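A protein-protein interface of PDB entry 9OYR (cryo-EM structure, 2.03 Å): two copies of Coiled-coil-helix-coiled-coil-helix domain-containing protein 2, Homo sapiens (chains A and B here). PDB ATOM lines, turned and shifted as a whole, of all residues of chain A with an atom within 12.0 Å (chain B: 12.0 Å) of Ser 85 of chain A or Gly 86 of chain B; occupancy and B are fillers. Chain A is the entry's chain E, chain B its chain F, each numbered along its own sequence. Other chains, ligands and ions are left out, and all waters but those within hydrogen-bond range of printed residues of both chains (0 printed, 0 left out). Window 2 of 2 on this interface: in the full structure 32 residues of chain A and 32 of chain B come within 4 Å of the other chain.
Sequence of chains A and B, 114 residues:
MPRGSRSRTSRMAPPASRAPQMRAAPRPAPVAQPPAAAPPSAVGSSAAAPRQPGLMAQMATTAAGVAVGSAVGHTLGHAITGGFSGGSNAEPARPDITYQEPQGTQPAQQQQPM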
ATOM      1  N   ILE A  80      14.992  14.343   3.196  1.00  0.00           N
ATOM      2  CA  ILE A  80      15.885  15.196   2.426  1.00  0.00           C
ATOM      3  C   ILE A  80      15.487  15.089   0.968  1.00  0.00           C
ATOM      4  O   ILE A  80      15.406  13.983   0.424  1.00  0.00           O
ATOM      5  CB  ILE A  80      17.363  14.812   2.610  1.00  0.00           C
ATOM      6  CG1 ILE A  80      17.768  14.924   4.077  1.00  0.00           C
ATOM      7  CG2 ILE A  80      18.244  15.677   1.736  1.00  0.00           C
ATOM      8  CD1 ILE A  80      18.930  14.046   4.451  1.00  0.00           C
ATOM      9  N   THR A  81      15.237  16.228   0.339  1.00  0.00           N
ATOM     10  CA  THR A  81      14.907  16.284  -1.072  1.00  0.00           C
ATOM     11  C   THR A  81      16.029  16.995  -1.806  1.00  0.00           C
ATOM     12  O   THR A  81      16.387  18.120  -1.453  1.00  0.00           O
ATOM     13  CB  THR A  81      13.583  17.012  -1.304  1.00  0.00           C
ATOM     14  OG1 THR A  81      12.551  16.394  -0.530  1.00  0.00           O
ATOM     15  CG2 THR A  81      13.207  16.950  -2.760  1.00  0.00           C
ATOM     16  N   GLY A  82      16.578  16.343  -2.824  1.00  0.00           N
ATOM     17  CA  GLY A  82      17.620  16.972  -3.612  1.00  0.00           C
ATOM     18  C   GLY A  82      17.058  18.083  -4.480  1.00  0.00           C
ATOM     19  O   GLY A  82      15.938  18.005  -4.981  1.00  0.00           O
ATOM     20  N   GLY A  83      17.857  19.125  -4.662  1.00  0.00           N
ATOM     21  CA  GLY A  83      17.497  20.241  -5.504  1.00  0.00           C
ATOM     22  C   GLY A  83      18.039  20.101  -6.909  1.00  0.00           C
ATOM     23  O   GLY A  83      18.337  19.004  -7.386  1.00  0.00           O
ATOM     24  N   PHE A  84      18.168  21.237  -7.579  1.00  0.00           N
ATOM     25  CA  PHE A  84      18.610  21.305  -8.965  1.00  0.00           C
ATOM     26  C   PHE A  84      19.954  22.016  -9.013  1.00  0.00           C
ATOM     27  O   PHE A  84      20.081  23.137  -8.514  1.00  0.00           O
ATOM     28  CB  PHE A  84      17.578  22.038  -9.821  1.00  0.00           C
ATOM     29  CG  PHE A  84      16.310  21.267 -10.029  1.00  0.00           C
ATOM     30  CD1 PHE A  84      15.406  21.107  -8.999  1.00  0.00           C
ATOM     31  CD2 PHE A  84      16.013  20.718 -11.260  1.00  0.00           C
ATOM     32  CE1 PHE A  84      14.246  20.401  -9.187  1.00  0.00           C
ATOM     33  CE2 PHE A  84      14.850  20.013 -11.450  1.00  0.00           C
ATOM     34  CZ  PHE A  84      13.969  19.854 -10.413  1.00  0.00           C
ATOM     35  N   SER A  85      20.947  21.371  -9.610  1.00  0.00           N
ATOM     36  CA  SER A  85      22.283  21.936  -9.724  1.00  0.00           C
ATOM     37  C   SER A  85      22.764  21.831 -11.163  1.00  0.00           C
ATOM     38  O   SER A  85      22.315  20.969 -11.919  1.00  0.00           O
ATOM     39  CB  SER A  85      23.265  21.237  -8.790  1.00  0.00           C
ATOM     40  OG  SER A  85      22.638  20.874  -7.579  1.00  0.00           O
ATOM     41  N   GLY A  86      23.678  22.720 -11.534  1.00  0.00           N
ATOM     42  CA  GLY A  86      24.200  22.764 -12.888  1.00  0.00           C
ATOM     43  C   GLY A  86      25.473  21.964 -13.085  1.00  0.00           C
ATOM     44  O   GLY A  86      26.076  21.492 -12.122  1.00  0.00           O
ATOM     45  N   THR B  81      15.654  11.730  -1.239  1.00  0.00           N
ATOM     46  CA  THR B  81      15.294  11.784  -2.644  1.00  0.00           C
ATOM     47  C   THR B  81      16.398  12.500  -3.401  1.00  0.00           C
ATOM     48  O   THR B  81      16.757  13.627  -3.055  1.00  0.00           O
ATOM     49  CB  THR B  81      13.961  12.506  -2.849  1.00  0.00           C
ATOM     50  OG1 THR B  81      12.950  11.883  -2.053  1.00  0.00           O
ATOM     51  CG2 THR B  81      13.556  12.440  -4.297  1.00  0.00           C
ATOM     52  N   GLY B  82      16.929  11.849  -4.429  1.00  0.00           N
ATOM     53  CA  GLY B  82      17.951  12.482  -5.239  1.00  0.00           C
ATOM     54  C   GLY B  82      17.368  13.591  -6.095  1.00  0.00           C
ATOM     55  O   GLY B  82      16.237  13.506  -6.574  1.00  0.00           O
ATOM     56  N   GLY B  83      18.156  14.635  -6.295  1.00  0.00           N
ATOM     57  CA  GLY B  83      17.775  15.750  -7.130  1.00  0.00           C
ATOM     58  C   GLY B  83      18.289  15.611  -8.545  1.00  0.00           C
ATOM     59  O   GLY B  83      18.583  14.515  -9.027  1.00  0.00           O
ATOM     60  N   PHE B  84      18.398  16.748  -9.219  1.00  0.00           N
ATOM     61  CA  PHE B  84      18.811  16.816 -10.614  1.00  0.00           C
ATOM     62  C   PHE B  84      20.150  17.534 -10.690  1.00  0.00           C
ATOM     63  O   PHE B  84      20.283  18.656 -10.194  1.00  0.00           O
ATOM     64  CB  PHE B  84      17.759  17.544 -11.449  1.00  0.00           C
ATOM     65  CG  PHE B  84      16.491  16.767 -11.631  1.00  0.00           C
ATOM     66  CD1 PHE B  84      15.609  16.603 -10.582  1.00  0.00           C
ATOM     67  CD2 PHE B  84      16.172  16.215 -12.855  1.00  0.00           C
ATOM     68  CE1 PHE B  84      14.448  15.891 -10.746  1.00  0.00           C
ATOM     69  CE2 PHE B  84      15.009  15.504 -13.021  1.00  0.00           C
ATOM     70  CZ  PHE B  84      14.149  15.342 -11.967  1.00  0.00           C
ATOM     71  N   SER B  85      21.135  16.894 -11.306  1.00  0.00           N
ATOM     72  CA  SER B  85      22.465  17.464 -11.447  1.00  0.00           C
ATOM     73  C   SER B  85      22.919  17.360 -12.895  1.00  0.00           C
ATOM     74  O   SER B  85      22.457  16.496 -13.643  1.00  0.00           O
ATOM     75  CB  SER B  85      23.470  16.772 -10.533  1.00  0.00           C
ATOM     76  OG  SER B  85      22.869  16.406  -9.310  1.00  0.00           O
ATOM     77  N   GLY B  86      23.820  18.253 -13.285  1.00  0.00           N
ATOM     78  CA  GLY B  86      24.313  18.299 -14.650  1.00  0.00           C
ATOM     79  C   GLY B  86      25.587  17.505 -14.872  1.00  0.00           C
ATOM     80  O   GLY B  86      26.210  17.037 -13.921  1.00  0.00           O
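The backbone carbonyl oxygen (O) of Ser 85 of chain A lies within hydrogen-bond range of the backbone NH (N) of Gly 86 of chain B (3.4 Å). O of Thr 81 of chain B is in hydrogen-bond range of N of Gly 82 of chain A (2.7 Å). The backbone carbonyl oxygen of Gly 83 of chain A is in hydrogen-bond range of the backbone NH of Phe 84 of chain B, 2.9 Å away. The backbone NH (N) of Ser 85 of chain A sits at hydrogen-bond distance from the backbone carbonyl oxygen (O) of Phe 84 of chain B, 2.9 Å away. O of Ile 80 of chain A is in hydrogen-bond range of N of Thr 81 of chain B.
Among the printed residues, pairs that only touch across the chains: Thr 81 of chain A with Thr 81 of chain B, Gly 82 of chain A with Gly 83 of chain B, Gly 83 of chain A with Gly 83 of chain B, Phe 84 of chain A with Phe 84 of chain B and Ser 85 of chain A with Ser 85 of chain B.
Gly 82 of chain A touches Thr 81 of chain B, but with the chains exchanged Thr 81 of chain A does not touch Gly 82 of chain B (5.6 Å). Gly 83 of chain A touches its own counterpart, Gly 83 of chain B. Gly 83 of chain A touches Phe 84 of chain B, but with the chains exchanged Phe 84 of chain A does not touch Gly 83 of chain B (5.5 Å). Ser 85 of chain A touches Phe 84 of chain B, but with the chains exchanged Phe 84 of chain A does not touch Ser 85 of chain B (5.6 Å). Positions printed for both chains: 81, 82, 83, 84, 85 and 86.
Printed residues of chain B within 4 Å of Ser 85 of chain A: Phe 84 (2.9 Å), Ser 85 (3.5 Å) and Gly 86 (3.4 Å). Gly 86 of chain B touches one residue of chain A. No residue of chain B comes within 4 Å of Gly 86 of chain A. Of chain A, only Gly 82 and Gly 83 come within 4 Å of Gly 83 of chain B. Of the printed residues of chain B, Thr 81 of chain A touches Thr 81 (3.7 Å). Printed residues of chain B within 4 Å of Gly 82 of chain A: Thr 81 (2.7 Å) and Gly 83 (3.6 Å). Gly 82 of chain B touches none of the printed residues of chain A. The nearest residue of chain A that does not touch Gly 86 of chain B is Gly 86 of chain A (4.1 Å). The nearest printed residue of chain B that does not touch Gly 82 of chain A is Gly 82 of chain B (4.2 Å).
Of the 6 printed residues of chain B, 5 touch a printed residue of chain A. Hydrophobic or aromatic side chains of chain B within 4 Å of the printed part of chain A: Phe 84. Along chain B the printed residues that touch a printed residue of chain A span positions 81 to 86.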
